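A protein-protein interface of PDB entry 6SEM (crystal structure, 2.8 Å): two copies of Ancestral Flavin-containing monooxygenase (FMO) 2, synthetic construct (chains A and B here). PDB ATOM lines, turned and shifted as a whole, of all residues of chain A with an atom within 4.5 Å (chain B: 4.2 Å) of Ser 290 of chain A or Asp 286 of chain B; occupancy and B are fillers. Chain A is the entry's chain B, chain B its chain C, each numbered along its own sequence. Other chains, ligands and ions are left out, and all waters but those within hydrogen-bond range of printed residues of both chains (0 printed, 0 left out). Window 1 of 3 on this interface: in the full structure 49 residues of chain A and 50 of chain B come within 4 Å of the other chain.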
ATOM      1  N   ASP A 287      -2.171  26.028   3.778  1.00  0.00           N
ATOM      2  CA  ASP A 287      -3.569  26.135   3.382  1.00  0.00           C
ATOM      3  C   ASP A 287      -4.296  27.195   4.225  1.00  0.00           C
ATOM      4  O   ASP A 287      -5.265  27.784   3.776  1.00  0.00           O
ATOM      5  CB  ASP A 287      -4.246  24.758   3.469  1.00  0.00           C
ATOM      6  CG  ASP A 287      -3.613  23.669   2.606  1.00  0.00           C
ATOM      7  OD1 ASP A 287      -2.649  23.027   3.039  1.00  0.00           O
ATOM      8  OD2 ASP A 287      -4.098  23.450   1.510  1.00  0.00           O
ATOM      9  N   LEU A 288      -3.834  27.440   5.446  1.00  0.00           N
ATOM     10  CA  LEU A 288      -4.619  28.183   6.437  1.00  0.00           C
ATOM     11  C   LEU A 288      -4.920  29.601   5.960  1.00  0.00           C
ATOM     12  O   LEU A 288      -6.072  30.005   5.971  1.00  0.00           O
ATOM     13  CB  LEU A 288      -3.871  28.219   7.770  1.00  0.00           C
ATOM     14  CG  LEU A 288      -4.580  28.987   8.891  1.00  0.00           C
ATOM     15  CD1 LEU A 288      -5.995  28.473   9.076  1.00  0.00           C
ATOM     16  CD2 LEU A 288      -3.814  28.904  10.200  1.00  0.00           C
ATOM     17  N   PRO A 289      -3.929  30.413   5.542  1.00  0.00           N
ATOM     18  CA  PRO A 289      -4.211  31.791   5.154  1.00  0.00           C
ATOM     19  C   PRO A 289      -5.296  31.847   4.062  1.00  0.00           C
ATOM     20  O   PRO A 289      -6.252  32.600   4.205  1.00  0.00           O
ATOM     21  CB  PRO A 289      -2.870  32.307   4.625  1.00  0.00           C
ATOM     22  CG  PRO A 289      -1.832  31.389   5.241  1.00  0.00           C
ATOM     23  CD  PRO A 289      -2.514  30.046   5.333  1.00  0.00           C
ATOM     24  N   SER A 290      -5.165  31.025   3.007  1.00  0.00           N
ATOM     25  CA  SER A 290      -6.174  30.953   1.924  1.00  0.00           C
ATOM     26  C   SER A 290      -7.545  30.610   2.514  1.00  0.00           C
ATOM     27  O   SER A 290      -8.559  31.254   2.225  1.00  0.00           O
ATOM     28  CB  SER A 290      -5.804  29.949   0.857  1.00  0.00           C
ATOM     29  OG  SER A 290      -6.137  28.626   1.267  1.00  0.00           O
ATOM     30  N   ARG A 291      -7.568  29.595   3.372  1.00  0.00           N
ATOM     31  CA  ARG A 291      -8.823  29.102   3.853  1.00  0.00           C
ATOM     32  C   ARG A 291      -9.483  30.174   4.741  1.00  0.00           C
ATOM     33  O   ARG A 291     -10.703  30.161   4.915  1.00  0.00           O
ATOM     34  CB  ARG A 291      -8.616  27.739   4.516  1.00  0.00           C
ATOM     35  CG  ARG A 291      -9.526  26.655   3.948  1.00  0.00           C
ATOM     36  CD  ARG A 291      -8.893  25.674   2.966  1.00  0.00           C
ATOM     37  NE  ARG A 291      -8.103  26.214   1.862  1.00  0.00           N
ATOM     38  CZ  ARG A 291      -7.593  25.448   0.889  1.00  0.00           C
ATOM     39  NH1 ARG A 291      -7.940  24.169   0.813  1.00  0.00           N
ATOM     40  NH2 ARG A 291      -6.738  25.955   0.008  1.00  0.00           N
ATOM     41  N   LEU A 292      -8.689  31.129   5.237  1.00  0.00           N
ATOM     42  CA  LEU A 292      -9.202  32.301   5.971  1.00  0.00           C
ATOM     43  C   LEU A 292      -9.791  33.325   4.995  1.00  0.00           C
ATOM     44  O   LEU A 292     -10.828  33.916   5.282  1.00  0.00           O
ATOM     45  CB  LEU A 292      -8.082  32.925   6.808  1.00  0.00           C
ATOM     46  CG  LEU A 292      -7.633  32.107   8.021  1.00  0.00           C
ATOM     47  CD1 LEU A 292      -6.302  32.601   8.574  1.00  0.00           C
ATOM     48  CD2 LEU A 292      -8.693  32.125   9.107  1.00  0.00           C
ATOM     49  N   LEU A 293      -9.133  33.531   3.847  1.00  0.00           N
ATOM     50  CA  LEU A 293      -9.651  34.439   2.822  1.00  0.00           C
ATOM     51  C   LEU A 293     -11.015  33.956   2.331  1.00  0.00           C
ATOM     52  O   LEU A 293     -11.949  34.745   2.254  1.00  0.00           O
ATOM     53  CB  LEU A 293      -8.690  34.538   1.638  1.00  0.00           C
ATOM     54  CG  LEU A 293      -7.876  35.826   1.563  1.00  0.00           C
ATOM     55  CD1 LEU A 293      -7.195  35.955   0.215  1.00  0.00           C
ATOM     56  CD2 LEU A 293      -8.738  37.043   1.834  1.00  0.00           C
ATOM     57  N   TYR A 294     -11.099  32.655   2.027  1.00  0.00           N
ATOM     58  CA  TYR A 294     -12.322  32.010   1.545  1.00  0.00           C
ATOM     59  C   TYR A 294     -13.432  32.116   2.594  1.00  0.00           C
ATOM     60  O   TYR A 294     -14.600  31.881   2.302  1.00  0.00           O
ATOM     61  CB  TYR A 294     -12.121  30.519   1.251  1.00  0.00           C
ATOM     62  CG  TYR A 294     -10.963  30.123   0.361  1.00  0.00           C
ATOM     63  CD1 TYR A 294     -10.175  31.045  -0.305  1.00  0.00           C
ATOM     64  CD2 TYR A 294     -10.681  28.784   0.152  1.00  0.00           C
ATOM     65  CE1 TYR A 294      -9.113  30.651  -1.104  1.00  0.00           C
ATOM     66  CE2 TYR A 294      -9.648  28.370  -0.672  1.00  0.00           C
ATOM     67  CZ  TYR A 294      -8.847  29.308  -1.298  1.00  0.00           C
ATOM     68  OH  TYR A 294      -7.814  28.916  -2.096  1.00  0.00           O
ATOM     69  N   SER B 222      -1.369  32.504  -6.812  1.00  0.00           N
ATOM     70  CA  SER B 222      -2.293  32.411  -5.700  1.00  0.00           C
ATOM     71  C   SER B 222      -3.150  33.669  -5.678  1.00  0.00           C
ATOM     72  O   SER B 222      -2.713  34.718  -6.111  1.00  0.00           O
ATOM     73  CB  SER B 222      -1.580  32.246  -4.399  1.00  0.00           C
ATOM     74  OG  SER B 222      -2.290  32.915  -3.365  1.00  0.00           O
ATOM     75  N   ARG B 223      -4.342  33.500  -5.105  1.00  0.00           N
ATOM     76  CA  ARG B 223      -5.340  34.574  -4.924  1.00  0.00           C
ATOM     77  C   ARG B 223      -4.770  35.546  -3.905  1.00  0.00           C
ATOM     78  O   ARG B 223      -5.157  36.711  -3.937  1.00  0.00           O
ATOM     79  CB  ARG B 223      -6.624  34.002  -4.332  1.00  0.00           C
ATOM     80  CG  ARG B 223      -7.267  32.899  -5.155  1.00  0.00           C
ATOM     81  CD  ARG B 223      -8.497  32.467  -4.407  1.00  0.00           C
ATOM     82  NE  ARG B 223      -9.473  31.798  -5.227  1.00  0.00           N
ATOM     83  CZ  ARG B 223      -9.291  30.619  -5.772  1.00  0.00           C
ATOM     84  NH1 ARG B 223      -8.153  29.987  -5.599  1.00  0.00           N
ATOM     85  NH2 ARG B 223     -10.242  30.070  -6.496  1.00  0.00           N
ATOM     86  N   ILE B 224      -3.924  35.032  -3.012  1.00  0.00           N
ATOM     87  CA  ILE B 224      -3.220  35.854  -2.013  1.00  0.00           C
ATOM     88  C   ILE B 224      -2.184  36.704  -2.745  1.00  0.00           C
ATOM     89  O   ILE B 224      -1.414  36.186  -3.565  1.00  0.00           O
ATOM     90  CB  ILE B 224      -2.469  34.994  -0.980  1.00  0.00           C
ATOM     91  CG1 ILE B 224      -3.305  33.836  -0.421  1.00  0.00           C
ATOM     92  CG2 ILE B 224      -1.894  35.868   0.116  1.00  0.00           C
ATOM     93  CD1 ILE B 224      -4.126  34.173   0.804  1.00  0.00           C
ATOM     94  N   TRP B 263       6.796  33.039  -5.720  1.00  0.00           N
ATOM     95  CA  TRP B 263       6.173  31.909  -5.028  1.00  0.00           C
ATOM     96  C   TRP B 263       7.073  30.675  -5.089  1.00  0.00           C
ATOM     97  O   TRP B 263       7.356  30.027  -4.085  1.00  0.00           O
ATOM     98  CB  TRP B 263       4.809  31.569  -5.628  1.00  0.00           C
ATOM     99  CG  TRP B 263       3.954  30.744  -4.721  1.00  0.00           C
ATOM    100  CD1 TRP B 263       4.241  30.375  -3.441  1.00  0.00           C
ATOM    101  CD2 TRP B 263       2.624  30.271  -4.982  1.00  0.00           C
ATOM    102  NE1 TRP B 263       3.189  29.691  -2.901  1.00  0.00           N
ATOM    103  CE2 TRP B 263       2.184  29.608  -3.826  1.00  0.00           C
ATOM    104  CE3 TRP B 263       1.757  30.351  -6.070  1.00  0.00           C
ATOM    105  CZ2 TRP B 263       0.936  28.998  -3.741  1.00  0.00           C
ATOM    106  CZ3 TRP B 263       0.516  29.761  -5.982  1.00  0.00           C
ATOM    107  CH2 TRP B 263       0.114  29.092  -4.830  1.00  0.00           C
ATOM    108  N   ASN B 285      -4.670  28.972  -8.292  1.00  0.00           N
ATOM    109  CA  ASN B 285      -4.786  27.884  -7.404  1.00  0.00           C
ATOM    110  C   ASN B 285      -3.811  28.158  -6.276  1.00  0.00           C
ATOM    111  O   ASN B 285      -2.623  28.264  -6.528  1.00  0.00           O
ATOM    112  CB  ASN B 285      -4.470  26.557  -8.094  1.00  0.00           C
ATOM    113  CG  ASN B 285      -5.048  25.397  -7.330  1.00  0.00           C
ATOM    114  OD1 ASN B 285      -4.533  25.073  -6.273  1.00  0.00           O
ATOM    115  ND2 ASN B 285      -6.138  24.810  -7.817  1.00  0.00           N
ATOM    116  N   ASP B 286      -4.332  28.286  -5.057  1.00  0.00           N
ATOM    117  CA  ASP B 286      -3.478  28.483  -3.891  1.00  0.00           C
ATOM    118  C   ASP B 286      -2.834  27.161  -3.432  1.00  0.00           C
ATOM    119  O   ASP B 286      -2.047  27.170  -2.517  1.00  0.00           O
ATOM    120  CB  ASP B 286      -4.270  29.063  -2.722  1.00  0.00           C
ATOM    121  CG  ASP B 286      -5.169  30.223  -3.111  1.00  0.00           C
ATOM    122  OD1 ASP B 286      -6.309  29.959  -3.514  1.00  0.00           O
ATOM    123  OD2 ASP B 286      -4.720  31.374  -3.006  1.00  0.00           O
ATOM    124  N   ASP B 287      -3.199  26.031  -4.053  1.00  0.00           N
ATOM    125  CA  ASP B 287      -2.963  24.700  -3.509  1.00  0.00           C
ATOM    126  C   ASP B 287      -1.939  23.931  -4.365  1.00  0.00           C
ATOM    127  O   ASP B 287      -1.214  23.082  -3.866  1.00  0.00           O
ATOM    128  CB  ASP B 287      -4.292  23.943  -3.349  1.00  0.00           C
ATOM    129  CG  ASP B 287      -5.315  24.645  -2.458  1.00  0.00           C
ATOM    130  OD1 ASP B 287      -6.093  25.474  -2.982  1.00  0.00           O
ATOM    131  OD2 ASP B 287      -5.317  24.391  -1.235  1.00  0.00           O
ATOM    132  N   LEU B 288      -1.849  24.258  -5.647  1.00  0.00           N
ATOM    133  CA  LEU B 288      -1.144  23.419  -6.610  1.00  0.00           C
ATOM    134  C   LEU B 288       0.338  23.285  -6.262  1.00  0.00           C
ATOM    135  O   LEU B 288       0.840  22.169  -6.179  1.00  0.00           O
ATOM    136  CB  LEU B 288      -1.320  24.001  -8.012  1.00  0.00           C
ATOM    137  CG  LEU B 288      -0.644  23.215  -9.121  1.00  0.00           C
ATOM    138  CD1 LEU B 288      -1.048  21.742  -9.052  1.00  0.00           C
ATOM    139  CD2 LEU B 288      -1.001  23.799 -10.482  1.00  0.00           C
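Of the 8 printed residues of chain B, 4 touch a printed residue of chain A.
Asp 287 of chain B touches its own counterpart, Asp 287 of chain A. Positions printed for both chains: 287 and 288.
The backbone carbonyl oxygen (O) of Asp 287 of chain A is in hydrogen-bond range of the side-chain hydroxyl (OG) of Ser 290 of chain A, at 2.8 Å. OD2 of Asp 287 of chain A lies within salt-bridge range of NH2 of Arg 291 of chain A (3.9 Å). The side-chain hydroxyl (OG) of Ser 222 of chain B sits at hydrogen-bond distance from the backbone NH (N) of Ile 224 of chain B (2.7 Å). The side-chain carboxylate of Asp 286 of chain B sits at hydrogen-bond distance from the side-chain hydroxyl of Ser 222 of chain B, at 2.9 Å. OD1 of Asp 286 of chain B is in salt-bridge range of NH1 of Arg 223 of chain B (2.8 Å). The side-chain amide oxygen (OD1) of Asn 285 of chain B lies within hydrogen-bond range of the backbone NH (N) of Asp 287 of chain B, 2.8 Å away.
NH2 of Arg 291 of chain A lies within salt-bridge range of OD2 of Asp 287 of chain B (2.5 Å). OD2 of Asp 287 of chain A lies close to OD2 of Asp 287 of chain B (3.1 Å). The side-chain carboxylate of Asp 286 of chain B sits close to the side-chain hydroxyl of Tyr 294 of chain A.
Of the printed residues of chain B, Ser 290 of chain A touches Ile 224 and Asp 286. Printed residues of chain A within 4 Å of Asp 286 of chain B: Ser 290 and Tyr 294. Printed residues of chain B within 4 Å of Asp 287 of chain A: Asp 287. Of the printed residues of chain B, Leu 293 of chain A touches Ile 224. Of the printed residues of chain B, Tyr 294 of chain A touches Arg 223 (3.7 Å), Asp 286 (2.3 Å) and Asp 287 (3.9 Å). Printed residues of chain A within 4 Å of Arg 223 of chain B: Tyr 294 (3.7 Å). The nearest printed residue of chain A that does not touch Asp 286 of chain B is Arg 291 of chain A (4.8 Å).
Among the printed residues, merely in contact across the chains: Leu 293 of chain A with Ile 224 of chain B (3.6 Å), Tyr 294 of chain A with Arg 223 of chain B (3.7 Å), Tyr 294 of chain A with Asp 287 of chain B (3.9 Å), Ser 290 of chain A with Ile 224 of chain B (3.98 Å) and Ser 290 of chain A with Asp 286 of chain B (3.99 Å).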
